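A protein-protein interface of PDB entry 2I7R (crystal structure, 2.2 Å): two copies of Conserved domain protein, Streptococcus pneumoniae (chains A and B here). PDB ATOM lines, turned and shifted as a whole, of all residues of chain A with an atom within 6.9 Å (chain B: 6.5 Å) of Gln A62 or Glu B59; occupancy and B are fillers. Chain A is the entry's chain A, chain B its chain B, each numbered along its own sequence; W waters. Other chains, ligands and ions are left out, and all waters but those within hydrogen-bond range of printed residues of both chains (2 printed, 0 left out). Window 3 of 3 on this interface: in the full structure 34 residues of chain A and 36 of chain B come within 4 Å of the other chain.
Water W1 lies within hydrogen-bond range of the backbone carbonyl oxygen (O) of Asn A60 (2.6 Å), the backbone NH (N) of Ser B63 (3.1 Å) and the side-chain amide nitrogen (NE2) of Gln A62 (3.4 Å). Water W2 lies within hydrogen-bond range of the backbone carbonyl oxygen (O) of Ser A63 (2.7 Å), the backbone carbonyl oxygen (O) of Ser B63 (2.8 Å), the backbone NH (N) of Gln B62 (3.1 Å) and the backbone NH (N) of Gln A62 (3.2 Å).
The backbone carbonyl oxygen of Ile A12 is in hydrogen-bond range of the backbone NH of Phe A61 (2.8 Å). O of Ile B12 sits at hydrogen-bond distance from N of Phe B61. The backbone carbonyl oxygen of Leu B58 lies within hydrogen-bond range of a ring nitrogen (ND1) of His B54 (2.8 Å). ND2 of Asn B60 sits at hydrogen-bond distance from NE2 of His B54 (3.0 Å).
Of the 12 printed residues of chain A, 8 touch a printed residue of chain B. Printed residues of chain A that touch a printed residue of chain B: Ile A11, Ile A12, Glu A59, Phe A61, Gln A62, Ser A63, Gly A64 and Ile A65. Hydrophobic or aromatic side chains of chain A that line the printed part of chain B: Ile A12, Phe A61 and Ile A65. Along chain A the printed residues that touch a printed residue of chain B span positions 11 to 65. Hydrophobic or aromatic side chains of chain B that line the printed part of chain A: Ile B12, Leu B58 and Phe B61. Among the printed residues, no Asp or Glu carboxylate lies within 4 Å of a Lys or Arg side-chain nitrogen of the other chain.
Phe A61 touches its own counterpart, Phe B61. Phe A61 touches Gly B64, and with the chains exchanged Gly A64 touches Phe B61. Gln A62 touches its own counterpart, Gln B62. Gly A64 touches Asn B60, but with the chains exchanged Asn A60 does not touch Gly B64 (4.1 Å). Of the 21 pairs that touch across the chains among the printed residues, 16 have their exchanged pair printed and touching as well.
Of chain B, only Glu B59 (3.2 Å), Gln B62 (3.1 Å) and Ser B63 (3.96 Å) come within 4 Å of Gln A62. Printed residues of chain B within 4 Å of Ser A63: Leu B58 (3.3 Å), Glu B59 (3.0 Å), Phe B61 (3.4 Å) and Gln B62 (3.8 Å). Ala A108 touches none of the printed residues of chain B. Printed residues of chain A within 4 Å of Ile B12: Gly A64 and Ile A65. Printed residues of chain A within 4 Å of Glu B59: Gln A62 (3.2 Å), Ser A63 (3.0 Å) and Gly A64 (3.0 Å). The nearest residue of chain B that does not touch Gln A62 is Gly B64 (5.7 Å).
Ile A11 touches Gly B64. CE1 of Phe B61 touches CE1 of Phe A61 (3.96 Å). Phe A61 touches Ser B63 (CA to O, 3.4 Å). Phe A61 touches Gly B64. Gln A62 touches Ser B63. Phe B61 touches Ser A63 (CA to O, 3.4 Å). Ser A63 touches Gln B62. Gly A64 touches Asn B60. CA of Gly A64 touches N of Phe B61, at 3.5 Å. Ile A65 touches Ile B12 (CA to CD1, 3.96 Å).
O of Gly B64 sits at hydrogen-bond distance from N of Ile A12 (2.8 Å). OE1 of Glu A59 is in hydrogen-bond range of NE2 of Gln B62 (2.9 Å). The backbone NH of Glu A59 lies within hydrogen-bond range of the side-chain hydroxyl of Ser B63. The backbone carbonyl oxygen (O) of Glu A59 lies close to the backbone NH (N) of Gly B64 (3.4 Å). The side-chain carboxylate of Glu B59 lies close to the side-chain amide oxygen of Gln A62 (3.2 Å). NE2 of Gln B62 sits close to NE2 of Gln A62. The backbone NH (N) of Ser A63 is in hydrogen-bond range of the side-chain carboxylate (OE1) of Glu B59. The backbone carbonyl oxygen (O) of Gly A64 is in hydrogen-bond range of the backbone NH (N) of Ile B12, 2.9 Å away. The backbone NH (N) of Gly A64 lies close to the backbone carbonyl oxygen (O) of Glu B59 (3.2 Å).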
ATOM      1  N   ILE A  11     -10.889  17.029 -27.868  1.00  0.00           N
ATOM      2  CA  ILE A  11     -11.784  16.438 -26.875  1.00  0.00           C
ATOM      3  C   ILE A  11     -12.965  17.395 -26.702  1.00  0.00           C
ATOM      4  O   ILE A  11     -12.776  18.586 -26.391  1.00  0.00           O
ATOM      5  CB  ILE A  11     -11.104  16.247 -25.465  1.00  0.00           C
ATOM      6  CG1 ILE A  11      -9.678  15.663 -25.574  1.00  0.00           C
ATOM      7  CG2 ILE A  11     -12.053  15.442 -24.519  1.00  0.00           C
ATOM      8  CD1 ILE A  11      -9.594  14.333 -26.357  1.00  0.00           C
ATOM      9  N   ILE A  12     -14.171  16.869 -26.894  1.00  0.00           N
ATOM     10  CA  ILE A  12     -15.386  17.678 -26.758  1.00  0.00           C
ATOM     11  C   ILE A  12     -15.869  17.569 -25.299  1.00  0.00           C
ATOM     12  O   ILE A  12     -16.119  16.445 -24.784  1.00  0.00           O
ATOM     13  CB  ILE A  12     -16.488  17.195 -27.700  1.00  0.00           C
ATOM     14  CG1 ILE A  12     -15.995  17.056 -29.133  1.00  0.00           C
ATOM     15  CG2 ILE A  12     -17.724  18.077 -27.601  1.00  0.00           C
ATOM     16  CD1 ILE A  12     -15.086  18.193 -29.584  1.00  0.00           C
ATOM     17  N   GLU A  59     -21.395  13.442 -29.267  1.00  0.00           N
ATOM     18  CA  GLU A  59     -21.669  13.698 -27.860  1.00  0.00           C
ATOM     19  C   GLU A  59     -20.410  14.195 -27.151  1.00  0.00           C
ATOM     20  O   GLU A  59     -19.310  14.049 -27.664  1.00  0.00           O
ATOM     21  CB  GLU A  59     -22.184  12.410 -27.213  1.00  0.00           C
ATOM     22  CG  GLU A  59     -23.341  11.797 -27.939  1.00  0.00           C
ATOM     23  CD  GLU A  59     -23.836  10.509 -27.282  1.00  0.00           C
ATOM     24  OE1 GLU A  59     -23.071   9.864 -26.552  1.00  0.00           O
ATOM     25  OE2 GLU A  59     -24.987  10.127 -27.496  1.00  0.00           O
ATOM     26  N   ASN A  60     -20.554  14.799 -25.984  1.00  0.00           N
ATOM     27  CA  ASN A  60     -19.382  15.062 -25.166  1.00  0.00           C
ATOM     28  C   ASN A  60     -18.663  13.764 -24.823  1.00  0.00           C
ATOM     29  O   ASN A  60     -19.257  12.644 -24.794  1.00  0.00           O
ATOM     30  CB  ASN A  60     -19.718  15.872 -23.904  1.00  0.00           C
ATOM     31  CG  ASN A  60     -20.284  17.252 -24.242  1.00  0.00           C
ATOM     32  OD1 ASN A  60     -20.164  17.728 -25.371  1.00  0.00           O
ATOM     33  ND2 ASN A  60     -20.932  17.863 -23.290  1.00  0.00           N
ATOM     34  N   PHE A  61     -17.363  13.925 -24.620  1.00  0.00           N
ATOM     35  CA  PHE A  61     -16.480  12.830 -24.340  1.00  0.00           C
ATOM     36  C   PHE A  61     -16.933  12.217 -23.044  1.00  0.00           C
ATOM     37  O   PHE A  61     -17.244  12.932 -22.115  1.00  0.00           O
ATOM     38  CB  PHE A  61     -15.021  13.306 -24.194  1.00  0.00           C
ATOM     39  CG  PHE A  61     -14.069  12.177 -23.885  1.00  0.00           C
ATOM     40  CD1 PHE A  61     -13.731  11.250 -24.876  1.00  0.00           C
ATOM     41  CD2 PHE A  61     -13.567  11.998 -22.604  1.00  0.00           C
ATOM     42  CE1 PHE A  61     -12.859  10.190 -24.600  1.00  0.00           C
ATOM     43  CE2 PHE A  61     -12.703  10.912 -22.309  1.00  0.00           C
ATOM     44  CZ  PHE A  61     -12.351  10.013 -23.299  1.00  0.00           C
ATOM     45  N   GLN A  62     -16.969  10.900 -23.008  1.00  0.00           N
ATOM     46  CA  GLN A  62     -17.229  10.150 -21.801  1.00  0.00           C
ATOM     47  C   GLN A  62     -15.966   9.421 -21.326  1.00  0.00           C
ATOM     48  O   GLN A  62     -15.316   9.837 -20.366  1.00  0.00           O
ATOM     49  CB  GLN A  62     -18.431   9.217 -22.024  1.00  0.00           C
ATOM     50  CG  GLN A  62     -19.766  10.045 -22.050  1.00  0.00           C
ATOM     51  CD  GLN A  62     -20.995   9.235 -22.423  1.00  0.00           C
ATOM     52  OE1 GLN A  62     -21.140   8.073 -22.016  1.00  0.00           O
ATOM     53  NE2 GLN A  62     -21.907   9.857 -23.205  1.00  0.00           N
ATOM     54  N   SER A  63     -15.590   8.346 -21.999  1.00  0.00           N
ATOM     55  CA  SER A  63     -14.424   7.581 -21.554  1.00  0.00           C
ATOM     56  C   SER A  63     -13.823   6.861 -22.754  1.00  0.00           C
ATOM     57  O   SER A  63     -14.248   7.081 -23.870  1.00  0.00           O
ATOM     58  CB  SER A  63     -14.813   6.591 -20.417  1.00  0.00           C
ATOM     59  OG  SER A  63     -13.667   6.156 -19.661  1.00  0.00           O
ATOM     60  N   GLY A  64     -12.821   6.022 -22.516  1.00  0.00           N
ATOM     61  CA  GLY A  64     -12.374   5.103 -23.549  1.00  0.00           C
ATOM     62  C   GLY A  64     -11.141   5.487 -24.324  1.00  0.00           C
ATOM     63  O   GLY A  64     -10.892   4.942 -25.371  1.00  0.00           O
ATOM     64  N   ILE A  65     -10.338   6.414 -23.818  1.00  0.00           N
ATOM     65  CA  ILE A  65      -9.054   6.653 -24.472  1.00  0.00           C
ATOM     66  C   ILE A  65      -7.923   6.782 -23.465  1.00  0.00           C
ATOM     67  O   ILE A  65      -8.150   7.056 -22.287  1.00  0.00           O
ATOM     68  CB  ILE A  65      -9.065   7.903 -25.419  1.00  0.00           C
ATOM     69  CG1 ILE A  65      -8.888   9.201 -24.609  1.00  0.00           C
ATOM     70  CG2 ILE A  65     -10.328   7.851 -26.392  1.00  0.00           C
ATOM     71  CD1 ILE A  65      -8.874  10.516 -25.449  1.00  0.00           C
ATOM     72  N   ALA A 108     -12.530  15.021 -16.893  1.00  0.00           N
ATOM     73  CA  ALA A 108     -13.533  14.697 -17.930  1.00  0.00           C
ATOM     74  C   ALA A 108     -13.442  13.297 -18.497  1.00  0.00           C
ATOM     75  O   ALA A 108     -13.775  13.070 -19.676  1.00  0.00           O
ATOM     76  CB  ALA A 108     -13.509  15.724 -19.077  1.00  0.00           C
ATOM     77  N   GLY A 109     -13.021  12.338 -17.669  1.00  0.00           N
ATOM     78  CA  GLY A 109     -12.905  10.957 -18.138  1.00  0.00           C
ATOM     79  C   GLY A 109     -11.566  10.659 -18.821  1.00  0.00           C
ATOM     80  O   GLY A 109     -11.299   9.491 -19.127  1.00  0.00           O
ATOM     81  N   LEU A 110     -10.717  11.675 -19.064  1.00  0.00           N
ATOM     82  CA  LEU A 110      -9.449  11.423 -19.806  1.00  0.00           C
ATOM     83  C   LEU A 110      -8.496  10.678 -18.907  1.00  0.00           C
ATOM     84  O   LEU A 110      -8.518  10.908 -17.702  1.00  0.00           O
ATOM     85  CB  LEU A 110      -8.745  12.694 -20.262  1.00  0.00           C
ATOM     86  CG  LEU A 110      -9.579  13.566 -21.202  1.00  0.00           C
ATOM     87  CD1 LEU A 110      -9.078  14.967 -21.201  1.00  0.00           C
ATOM     88  CD2 LEU A 110      -9.603  12.941 -22.551  1.00  0.00           C
ATOM     89  N   ILE B  12     -10.189   2.503 -26.711  1.00  0.00           N
ATOM     90  CA  ILE B  12     -10.701   1.269 -26.100  1.00  0.00           C
ATOM     91  C   ILE B  12     -12.033   0.913 -26.746  1.00  0.00           C
ATOM     92  O   ILE B  12     -13.021   1.632 -26.603  1.00  0.00           O
ATOM     93  CB  ILE B  12     -10.846   1.380 -24.573  1.00  0.00           C
ATOM     94  CG1 ILE B  12      -9.504   1.614 -23.859  1.00  0.00           C
ATOM     95  CG2 ILE B  12     -11.351   0.035 -24.010  1.00  0.00           C
ATOM     96  CD1 ILE B  12      -8.582   2.721 -24.385  1.00  0.00           C
ATOM     97  N   HIS B  54      -8.537  -3.171 -20.844  1.00  0.00           N
ATOM     98  CA  HIS B  54      -8.536  -1.969 -20.035  1.00  0.00           C
ATOM     99  C   HIS B  54      -7.278  -1.951 -19.173  1.00  0.00           C
ATOM    100  O   HIS B  54      -7.272  -2.483 -18.048  1.00  0.00           O
ATOM    101  CB  HIS B  54      -9.807  -1.912 -19.165  1.00  0.00           C
ATOM    102  CG  HIS B  54     -11.077  -1.784 -19.953  1.00  0.00           C
ATOM    103  ND1 HIS B  54     -12.262  -1.357 -19.393  1.00  0.00           N
ATOM    104  CD2 HIS B  54     -11.342  -2.019 -21.260  1.00  0.00           C
ATOM    105  CE1 HIS B  54     -13.204  -1.338 -20.321  1.00  0.00           C
ATOM    106  NE2 HIS B  54     -12.673  -1.736 -21.462  1.00  0.00           N
ATOM    107  N   PRO B  57      -8.934   1.163 -15.196  1.00  0.00           N
ATOM    108  CA  PRO B  57     -10.398   1.149 -15.345  1.00  0.00           C
ATOM    109  C   PRO B  57     -10.935   2.339 -16.154  1.00  0.00           C
ATOM    110  O   PRO B  57     -10.450   3.473 -15.993  1.00  0.00           O
ATOM    111  CB  PRO B  57     -10.915   1.183 -13.896  1.00  0.00           C
ATOM    112  CG  PRO B  57      -9.789   1.819 -13.089  1.00  0.00           C
ATOM    113  CD  PRO B  57      -8.499   1.572 -13.839  1.00  0.00           C
ATOM    114  N   LEU B  58     -11.923   2.050 -17.013  1.00  0.00           N
ATOM    115  CA  LEU B  58     -12.597   3.009 -17.920  1.00  0.00           C
ATOM    116  C   LEU B  58     -13.657   2.262 -18.772  1.00  0.00           C
ATOM    117  O   LEU B  58     -13.622   1.041 -18.842  1.00  0.00           O
ATOM    118  CB  LEU B  58     -11.561   3.724 -18.827  1.00  0.00           C
ATOM    119  CG  LEU B  58     -10.428   2.916 -19.466  1.00  0.00           C
ATOM    120  CD1 LEU B  58     -10.985   1.841 -20.388  1.00  0.00           C
ATOM    121  CD2 LEU B  58      -9.400   3.818 -20.188  1.00  0.00           C
ATOM    122  N   GLU B  59     -14.585   3.002 -19.399  1.00  0.00           N
ATOM    123  CA  GLU B  59     -15.613   2.464 -20.338  1.00  0.00           C
ATOM    124  C   GLU B  59     -15.005   2.341 -21.764  1.00  0.00           C
ATOM    125  O   GLU B  59     -14.077   3.067 -22.112  1.00  0.00           O
ATOM    126  CB  GLU B  59     -16.868   3.407 -20.316  1.00  0.00           C
ATOM    127  CG  GLU B  59     -17.675   3.692 -21.693  1.00  0.00           C
ATOM    128  CD  GLU B  59     -18.024   5.231 -21.968  1.00  0.00           C
ATOM    129  OE1 GLU B  59     -17.262   5.920 -22.764  1.00  0.00           O
ATOM    130  OE2 GLU B  59     -19.072   5.712 -21.409  1.00  0.00           O
ATOM    131  N   ASN B  60     -15.497   1.423 -22.584  1.00  0.00           N
ATOM    132  CA  ASN B  60     -15.179   1.508 -24.000  1.00  0.00           C
ATOM    133  C   ASN B  60     -15.427   2.931 -24.544  1.00  0.00           C
ATOM    134  O   ASN B  60     -16.347   3.655 -24.085  1.00  0.00           O
ATOM    135  CB  ASN B  60     -15.979   0.487 -24.823  1.00  0.00           C
ATOM    136  CG  ASN B  60     -15.525  -0.975 -24.579  1.00  0.00           C
ATOM    137  OD1 ASN B  60     -16.075  -1.883 -25.172  1.00  0.00           O
ATOM    138  ND2 ASN B  60     -14.552  -1.186 -23.719  1.00  0.00           N
ATOM    139  N   PHE B  61     -14.610   3.344 -25.509  1.00  0.00           N
ATOM    140  CA  PHE B  61     -14.833   4.624 -26.158  1.00  0.00           C
ATOM    141  C   PHE B  61     -16.287   4.753 -26.625  1.00  0.00           C
ATOM    142  O   PHE B  61     -16.832   3.788 -27.221  1.00  0.00           O
ATOM    143  CB  PHE B  61     -13.935   4.801 -27.373  1.00  0.00           C
ATOM    144  CG  PHE B  61     -14.146   6.120 -28.047  1.00  0.00           C
ATOM    145  CD1 PHE B  61     -13.695   7.293 -27.445  1.00  0.00           C
ATOM    146  CD2 PHE B  61     -14.880   6.202 -29.229  1.00  0.00           C
ATOM    147  CE1 PHE B  61     -13.928   8.550 -28.045  1.00  0.00           C
ATOM    148  CE2 PHE B  61     -15.129   7.454 -29.838  1.00  0.00           C
ATOM    149  CZ  PHE B  61     -14.652   8.628 -29.252  1.00  0.00           C
ATOM    150  N   GLN B  62     -16.893   5.931 -26.405  1.00  0.00           N
ATOM    151  CA  GLN B  62     -18.232   6.194 -27.006  1.00  0.00           C
ATOM    152  C   GLN B  62     -18.254   7.285 -28.122  1.00  0.00           C
ATOM    153  O   GLN B  62     -18.498   7.012 -29.300  1.00  0.00           O
ATOM    154  CB  GLN B  62     -19.256   6.488 -25.898  1.00  0.00           C
ATOM    155  CG  GLN B  62     -20.704   6.789 -26.362  1.00  0.00           C
ATOM    156  CD  GLN B  62     -21.704   6.551 -25.233  1.00  0.00           C
ATOM    157  OE1 GLN B  62     -21.597   5.562 -24.508  1.00  0.00           O
ATOM    158  NE2 GLN B  62     -22.646   7.470 -25.060  1.00  0.00           N
ATOM    159  N   SER B  63     -18.011   8.521 -27.716  1.00  0.00           N
ATOM    160  CA  SER B  63     -18.025   9.663 -28.618  1.00  0.00           C
ATOM    161  C   SER B  63     -17.136  10.752 -28.031  1.00  0.00           C
ATOM    162  O   SER B  63     -16.557  10.586 -26.938  1.00  0.00           O
ATOM    163  CB  SER B  63     -19.485  10.193 -28.794  1.00  0.00           C
ATOM    164  OG  SER B  63     -19.592  10.996 -29.958  1.00  0.00           O
ATOM    165  N   GLY B  64     -17.024  11.859 -28.769  1.00  0.00           N
ATOM    166  CA  GLY B  64     -16.500  13.090 -28.224  1.00  0.00           C
ATOM    167  C   GLY B  64     -15.055  13.407 -28.487  1.00  0.00           C
ATOM    168  O   GLY B  64     -14.476  14.173 -27.739  1.00  0.00           O
HETATM  169  O   HOH W   1     -19.446  10.135 -25.562  1.00  0.00           O
HETATM  170  O   HOH W   2     -16.065   8.600 -25.082  1.00  0.00           O
